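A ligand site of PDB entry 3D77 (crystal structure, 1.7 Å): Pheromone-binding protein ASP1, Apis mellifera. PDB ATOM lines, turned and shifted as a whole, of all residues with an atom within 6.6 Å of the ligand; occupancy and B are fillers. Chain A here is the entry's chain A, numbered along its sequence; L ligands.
An oxygen (O1) of the ligand sits at hydrogen-bond distance from the backbone NH of Ile 119 (3.0 Å).
N1 of the ligand lies within hydrogen-bond range of O of Phe 117.
The chain-end carboxylate of Ile 119 lies within hydrogen-bond range of the side-chain hydroxyl of Tyr 48 (2.6 Å).
The side-chain sulfur (SD) of Met 49 is in hydrogen-bond range of the indole nitrogen (NE1) of Trp 116 (3.6 Å).
O of Leu 53 lies within hydrogen-bond range of N of Leu 58, at 2.9 Å.
Residues that only touch the ligand: Trp 4, Leu 52, Leu 53, Phe 56, Leu 58, Val 115, Trp 116 and Val 118.
Within 4 Å of the ligand: Trp 4, Leu 52, Leu 53, Phe 56, Leu 58, Val 115, Trp 116, Phe 117, Val 118 and Ile 119.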
ATOM      1  N   TRP A   4      17.181  -9.989  -3.706  1.00  0.00           N
ATOM      2  CA  TRP A   4      16.539 -11.273  -4.116  1.00  0.00           C
ATOM      3  C   TRP A   4      16.905 -12.413  -3.180  1.00  0.00           C
ATOM      4  O   TRP A   4      16.494 -13.550  -3.402  1.00  0.00           O
ATOM      5  CB  TRP A   4      16.947 -11.639  -5.558  1.00  0.00           C
ATOM      6  CG  TRP A   4      18.386 -11.365  -5.799  1.00  0.00           C
ATOM      7  CD1 TRP A   4      18.935 -10.241  -6.362  1.00  0.00           C
ATOM      8  CD2 TRP A   4      19.500 -12.202  -5.439  1.00  0.00           C
ATOM      9  NE1 TRP A   4      20.300 -10.339  -6.391  1.00  0.00           N
ATOM     10  CE2 TRP A   4      20.673 -11.524  -5.831  1.00  0.00           C
ATOM     11  CE3 TRP A   4      19.597 -13.462  -4.843  1.00  0.00           C
ATOM     12  CZ2 TRP A   4      21.946 -12.062  -5.637  1.00  0.00           C
ATOM     13  CZ3 TRP A   4      20.854 -13.999  -4.642  1.00  0.00           C
ATOM     14  CH2 TRP A   4      22.015 -13.292  -5.043  1.00  0.00           C
ATOM     15  N   VAL A   5      17.704 -12.134  -2.153  1.00  0.00           N
ATOM     16  CA  VAL A   5      18.199 -13.218  -1.304  1.00  0.00           C
ATOM     17  C   VAL A   5      17.066 -13.760  -0.428  1.00  0.00           C
ATOM     18  O   VAL A   5      16.475 -12.992   0.314  1.00  0.00           O
ATOM     19  CB  VAL A   5      19.360 -12.735  -0.438  1.00  0.00           C
ATOM     20  CG1 VAL A   5      19.777 -13.813   0.528  1.00  0.00           C
ATOM     21  CG2 VAL A   5      20.549 -12.307  -1.328  1.00  0.00           C
ATOM     22  N   VAL A   9      19.196 -18.074   3.417  1.00  0.00           N
ATOM     23  CA  VAL A   9      20.595 -17.664   3.504  1.00  0.00           C
ATOM     24  C   VAL A   9      20.946 -16.986   4.822  1.00  0.00           C
ATOM     25  O   VAL A   9      21.981 -17.287   5.413  1.00  0.00           O
ATOM     26  CB  VAL A   9      20.913 -16.637   2.405  1.00  0.00           C
ATOM     27  CG1 VAL A   9      20.348 -17.094   1.062  1.00  0.00           C
ATOM     28  CG2 VAL A   9      20.341 -15.280   2.791  1.00  0.00           C
ATOM     29  N   VAL A  13      24.243 -17.767   7.200  1.00  0.00           N
ATOM     30  CA  VAL A  13      25.377 -16.878   6.940  1.00  0.00           C
ATOM     31  C   VAL A  13      25.775 -16.016   8.144  1.00  0.00           C
ATOM     32  O   VAL A  13      26.818 -15.368   8.127  1.00  0.00           O
ATOM     33  CB  VAL A  13      25.025 -15.948   5.728  1.00  0.00           C
ATOM     34  CG1 VAL A  13      25.943 -14.724   5.639  1.00  0.00           C
ATOM     35  CG2 VAL A  13      25.084 -16.748   4.428  1.00  0.00           C
ATOM     36  N   TYR A  48      35.829  -7.733   3.025  1.00  0.00           N
ATOM     37  CA  TYR A  48      34.595  -8.324   3.552  1.00  0.00           C
ATOM     38  C   TYR A  48      33.912  -9.137   2.450  1.00  0.00           C
ATOM     39  O   TYR A  48      33.530 -10.283   2.636  1.00  0.00           O
ATOM     40  CB  TYR A  48      33.657  -7.238   4.091  1.00  0.00           C
ATOM     41  CG  TYR A  48      32.308  -7.808   4.482  1.00  0.00           C
ATOM     42  CD1 TYR A  48      32.152  -8.486   5.688  1.00  0.00           C
ATOM     43  CD2 TYR A  48      31.222  -7.752   3.618  1.00  0.00           C
ATOM     44  CE1 TYR A  48      30.923  -9.050   6.032  1.00  0.00           C
ATOM     45  CE2 TYR A  48      29.999  -8.293   3.969  1.00  0.00           C
ATOM     46  CZ  TYR A  48      29.878  -8.963   5.150  1.00  0.00           C
ATOM     47  OH  TYR A  48      28.640  -9.532   5.503  1.00  0.00           O
ATOM     48  N   MET A  49      33.791  -8.561   1.254  1.00  0.00           N
ATOM     49  CA  MET A  49      33.169  -9.293   0.137  1.00  0.00           C
ATOM     50  C   MET A  49      33.965 -10.551  -0.218  1.00  0.00           C
ATOM     51  O   MET A  49      33.393 -11.624  -0.407  1.00  0.00           O
ATOM     52  CB  MET A  49      33.002  -8.383  -1.059  1.00  0.00           C
ATOM     53  CG  MET A  49      32.040  -7.210  -0.797  1.00  0.00           C
ATOM     54  SD  MET A  49      31.656  -6.214  -2.283  1.00  0.00           S
ATOM     55  CE  MET A  49      33.262  -5.465  -2.633  1.00  0.00           C
ATOM     56  N   LEU A  52      33.288 -13.220   2.590  1.00  0.00           N
ATOM     57  CA  LEU A  52      32.000 -13.902   2.536  1.00  0.00           C
ATOM     58  C   LEU A  52      31.902 -14.842   1.325  1.00  0.00           C
ATOM     59  O   LEU A  52      31.381 -15.958   1.452  1.00  0.00           O
ATOM     60  CB  LEU A  52      30.880 -12.879   2.606  1.00  0.00           C
ATOM     61  CG  LEU A  52      29.578 -13.373   3.232  1.00  0.00           C
ATOM     62  CD1 LEU A  52      29.706 -13.559   4.732  1.00  0.00           C
ATOM     63  CD2 LEU A  52      28.517 -12.331   2.891  1.00  0.00           C
ATOM     64  N   LEU A  53      32.442 -14.445   0.165  1.00  0.00           N
ATOM     65  CA  LEU A  53      32.513 -15.358  -0.992  1.00  0.00           C
ATOM     66  C   LEU A  53      33.301 -16.622  -0.623  1.00  0.00           C
ATOM     67  O   LEU A  53      32.909 -17.733  -0.993  1.00  0.00           O
ATOM     68  CB  LEU A  53      33.095 -14.659  -2.219  1.00  0.00           C
ATOM     69  CG  LEU A  53      32.289 -13.545  -2.853  1.00  0.00           C
ATOM     70  CD1 LEU A  53      33.108 -12.706  -3.857  1.00  0.00           C
ATOM     71  CD2 LEU A  53      31.027 -14.129  -3.531  1.00  0.00           C
ATOM     72  N   PHE A  56      31.310 -19.043   1.457  1.00  0.00           N
ATOM     73  CA  PHE A  56      30.284 -19.768   0.676  1.00  0.00           C
ATOM     74  C   PHE A  56      30.890 -20.674  -0.411  1.00  0.00           C
ATOM     75  O   PHE A  56      30.157 -21.182  -1.277  1.00  0.00           O
ATOM     76  CB  PHE A  56      29.351 -18.767  -0.004  1.00  0.00           C
ATOM     77  CG  PHE A  56      28.720 -17.746   0.936  1.00  0.00           C
ATOM     78  CD1 PHE A  56      28.588 -17.993   2.304  1.00  0.00           C
ATOM     79  CD2 PHE A  56      28.244 -16.543   0.411  1.00  0.00           C
ATOM     80  CE1 PHE A  56      27.993 -17.050   3.122  1.00  0.00           C
ATOM     81  CE2 PHE A  56      27.648 -15.599   1.230  1.00  0.00           C
ATOM     82  CZ  PHE A  56      27.525 -15.855   2.592  1.00  0.00           C
ATOM     83  N   LEU A  58      32.676 -19.841  -2.995  1.00  0.00           N
ATOM     84  CA  LEU A  58      32.477 -19.269  -4.292  1.00  0.00           C
ATOM     85  C   LEU A  58      33.755 -18.737  -4.912  1.00  0.00           C
ATOM     86  O   LEU A  58      33.773 -18.418  -6.102  1.00  0.00           O
ATOM     87  CB  LEU A  58      31.491 -18.112  -4.179  1.00  0.00           C
ATOM     88  CG  LEU A  58      30.056 -18.521  -3.792  1.00  0.00           C
ATOM     89  CD1 LEU A  58      29.189 -17.299  -3.823  1.00  0.00           C
ATOM     90  CD2 LEU A  58      29.513 -19.612  -4.705  1.00  0.00           C
ATOM     91  N   MET A  70      28.239 -20.180  -8.005  1.00  0.00           N
ATOM     92  CA  MET A  70      27.664 -18.858  -7.854  1.00  0.00           C
ATOM     93  C   MET A  70      26.302 -18.822  -8.525  1.00  0.00           C
ATOM     94  O   MET A  70      25.349 -18.368  -7.933  1.00  0.00           O
ATOM     95  CB  MET A  70      28.552 -17.796  -8.471  1.00  0.00           C
ATOM     96  CG  MET A  70      28.101 -16.374  -8.167  1.00  0.00           C
ATOM     97  SD  MET A  70      29.207 -15.104  -8.821  1.00  0.00           S
ATOM     98  CE  MET A  70      30.230 -14.834  -7.383  1.00  0.00           C
ATOM     99  N   LEU A  73      23.260 -20.431  -6.638  1.00  0.00           N
ATOM    100  CA  LEU A  73      22.691 -19.736  -5.485  1.00  0.00           C
ATOM    101  C   LEU A  73      21.778 -18.546  -5.846  1.00  0.00           C
ATOM    102  O   LEU A  73      21.218 -17.899  -4.953  1.00  0.00           O
ATOM    103  CB  LEU A  73      23.824 -19.254  -4.562  1.00  0.00           C
ATOM    104  CG  LEU A  73      24.674 -20.369  -3.960  1.00  0.00           C
ATOM    105  CD1 LEU A  73      25.885 -19.821  -3.222  1.00  0.00           C
ATOM    106  CD2 LEU A  73      23.809 -21.189  -3.013  1.00  0.00           C
ATOM    107  N   LEU A  74      21.616 -18.242  -7.138  1.00  0.00           N
ATOM    108  CA  LEU A  74      20.805 -17.126  -7.594  1.00  0.00           C
ATOM    109  C   LEU A  74      19.425 -17.636  -8.012  1.00  0.00           C
ATOM    110  O   LEU A  74      19.305 -18.782  -8.426  1.00  0.00           O
ATOM    111  CB  LEU A  74      21.488 -16.444  -8.784  1.00  0.00           C
ATOM    112  CG  LEU A  74      22.882 -15.875  -8.523  1.00  0.00           C
ATOM    113  CD1 LEU A  74      23.606 -15.622  -9.818  1.00  0.00           C
ATOM    114  CD2 LEU A  74      22.757 -14.584  -7.715  1.00  0.00           C
ATOM    115  N   MET A  86      28.723 -12.257 -15.919  1.00  0.00           N
ATOM    116  CA  MET A  86      29.903 -12.990 -15.566  1.00  0.00           C
ATOM    117  C   MET A  86      30.773 -13.405 -16.743  1.00  0.00           C
ATOM    118  O   MET A  86      31.960 -13.568 -16.631  1.00  0.00           O
ATOM    119  CB  MET A  86      29.567 -14.182 -14.666  1.00  0.00           C
ATOM    120  CG  MET A  86      28.997 -13.791 -13.310  1.00  0.00           C
ATOM    121  SD  MET A  86      30.154 -12.891 -12.253  1.00  0.00           S
ATOM    122  CE  MET A  86      29.068 -12.210 -11.060  1.00  0.00           C
ATOM    123  N   ILE A 101      38.057  -8.707  -5.978  1.00  0.00           N
ATOM    124  CA  ILE A 101      36.604  -8.650  -5.782  1.00  0.00           C
ATOM    125  C   ILE A 101      36.051  -7.231  -5.952  1.00  0.00           C
ATOM    126  O   ILE A 101      34.929  -7.056  -6.472  1.00  0.00           O
ATOM    127  CB  ILE A 101      36.204  -9.324  -4.434  1.00  0.00           C
ATOM    128  CG1 ILE A 101      36.658 -10.797  -4.401  1.00  0.00           C
ATOM    129  CG2 ILE A 101      34.675  -9.217  -4.193  1.00  0.00           C
ATOM    130  CD1 ILE A 101      36.325 -11.666  -5.630  1.00  0.00           C
ATOM    131  N   VAL A 108      30.383  -5.744 -12.451  1.00  0.00           N
ATOM    132  CA  VAL A 108      28.999  -6.216 -12.384  1.00  0.00           C
ATOM    133  C   VAL A 108      28.020  -5.067 -12.204  1.00  0.00           C
ATOM    134  O   VAL A 108      27.028  -4.965 -12.940  1.00  0.00           O
ATOM    135  CB  VAL A 108      28.811  -7.276 -11.279  1.00  0.00           C
ATOM    136  CG1 VAL A 108      27.326  -7.645 -11.122  1.00  0.00           C
ATOM    137  CG2 VAL A 108      29.650  -8.493 -11.570  1.00  0.00           C
ATOM    138  N   VAL A 115      22.261  -7.589  -9.927  1.00  0.00           N
ATOM    139  CA  VAL A 115      22.947  -8.845  -9.678  1.00  0.00           C
ATOM    140  C   VAL A 115      23.801  -8.784  -8.411  1.00  0.00           C
ATOM    141  O   VAL A 115      23.770  -9.700  -7.617  1.00  0.00           O
ATOM    142  CB  VAL A 115      23.826  -9.255 -10.864  1.00  0.00           C
ATOM    143  CG1 VAL A 115      24.539 -10.555 -10.578  1.00  0.00           C
ATOM    144  CG2 VAL A 115      22.945  -9.403 -12.138  1.00  0.00           C
ATOM    145  N   TRP A 116      24.547  -7.705  -8.225  1.00  0.00           N
ATOM    146  CA  TRP A 116      25.536  -7.679  -7.129  1.00  0.00           C
ATOM    147  C   TRP A 116      24.950  -7.215  -5.803  1.00  0.00           C
ATOM    148  O   TRP A 116      24.854  -6.030  -5.521  1.00  0.00           O
ATOM    149  CB  TRP A 116      26.764  -6.841  -7.513  1.00  0.00           C
ATOM    150  CG  TRP A 116      27.918  -7.128  -6.593  1.00  0.00           C
ATOM    151  CD1 TRP A 116      28.237  -6.471  -5.446  1.00  0.00           C
ATOM    152  CD2 TRP A 116      28.877  -8.169  -6.749  1.00  0.00           C
ATOM    153  NE1 TRP A 116      29.357  -7.031  -4.873  1.00  0.00           N
ATOM    154  CE2 TRP A 116      29.774  -8.079  -5.636  1.00  0.00           C
ATOM    155  CE3 TRP A 116      29.096  -9.168  -7.695  1.00  0.00           C
ATOM    156  CZ2 TRP A 116      30.844  -8.954  -5.466  1.00  0.00           C
ATOM    157  CZ3 TRP A 116      30.167 -10.030  -7.528  1.00  0.00           C
ATOM    158  CH2 TRP A 116      31.028  -9.916  -6.418  1.00  0.00           C
ATOM    159  N   PHE A 117      24.599  -8.174  -4.969  1.00  0.00           N
ATOM    160  CA  PHE A 117      24.082  -7.894  -3.649  1.00  0.00           C
ATOM    161  C   PHE A 117      25.030  -8.457  -2.642  1.00  0.00           C
ATOM    162  O   PHE A 117      25.511  -9.596  -2.803  1.00  0.00           O
ATOM    163  CB  PHE A 117      22.712  -8.540  -3.446  1.00  0.00           C
ATOM    164  CG  PHE A 117      22.105  -8.269  -2.082  1.00  0.00           C
ATOM    165  CD1 PHE A 117      21.543  -7.035  -1.793  1.00  0.00           C
ATOM    166  CD2 PHE A 117      22.123  -9.238  -1.086  1.00  0.00           C
ATOM    167  CE1 PHE A 117      20.984  -6.768  -0.543  1.00  0.00           C
ATOM    168  CE2 PHE A 117      21.576  -8.969   0.177  1.00  0.00           C
ATOM    169  CZ  PHE A 117      21.028  -7.720   0.434  1.00  0.00           C
ATOM    170  N   VAL A 118      25.272  -7.706  -1.576  1.00  0.00           N
ATOM    171  CA  VAL A 118      26.165  -8.155  -0.555  1.00  0.00           C
ATOM    172  C   VAL A 118      25.373  -8.367   0.715  1.00  0.00           C
ATOM    173  O   VAL A 118      24.684  -7.465   1.185  1.00  0.00           O
ATOM    174  CB  VAL A 118      27.280  -7.111  -0.328  1.00  0.00           C
ATOM    175  CG1 VAL A 118      28.115  -7.447   0.907  1.00  0.00           C
ATOM    176  CG2 VAL A 118      28.091  -6.990  -1.616  1.00  0.00           C
ATOM    177  N   ILE A 119      25.457  -9.568   1.274  1.00  0.00           N
ATOM    178  CA  ILE A 119      24.779  -9.841   2.553  1.00  0.00           C
ATOM    179  C   ILE A 119      25.513  -9.195   3.694  1.00  0.00           C
ATOM    180  O   ILE A 119      26.735  -9.335   3.778  1.00  0.00           O
ATOM    181  CB  ILE A 119      24.688 -11.344   2.813  1.00  0.00           C
ATOM    182  CG1 ILE A 119      23.666 -11.983   1.856  1.00  0.00           C
ATOM    183  CG2 ILE A 119      24.403 -11.623   4.310  1.00  0.00           C
ATOM    184  CD1 ILE A 119      23.792 -13.504   1.770  1.00  0.00           C
ATOM    185  OXT ILE A 119      24.916  -8.567   4.592  1.00  0.00           O
HETATM  186  O1  LIG L   1      26.797 -11.841  -0.179  1.00  0.00           O
HETATM  187  S1  LIG L   1      27.359 -12.413  -1.434  1.00  0.00           S
HETATM  188  O2  LIG L   1      28.677 -12.986  -1.085  1.00  0.00           O
HETATM  189  N1  LIG L   1      27.439 -11.257  -2.449  1.00  0.00           N
HETATM  190  C1  LIG L   1      28.455 -11.122  -3.493  1.00  0.00           C
HETATM  191  C2  LIG L   1      28.051 -12.007  -4.672  1.00  0.00           C
HETATM  192  C3  LIG L   1      26.788 -11.526  -5.377  1.00  0.00           C
HETATM  193  C4  LIG L   1      26.552 -12.236  -6.692  1.00  0.00           C
HETATM  194  C5  LIG L   1      26.340 -13.535  -1.979  1.00  0.00           C
HETATM  195  C6  LIG L   1      26.793 -14.754  -2.486  1.00  0.00           C
HETATM  196  C7  LIG L   1      25.882 -15.702  -2.971  1.00  0.00           C
HETATM  197  C8  LIG L   1      24.515 -15.443  -2.967  1.00  0.00           C
HETATM  198  C9  LIG L   1      24.064 -14.226  -2.470  1.00  0.00           C
HETATM  199  C10 LIG L   1      24.973 -13.276  -1.976  1.00  0.00           C
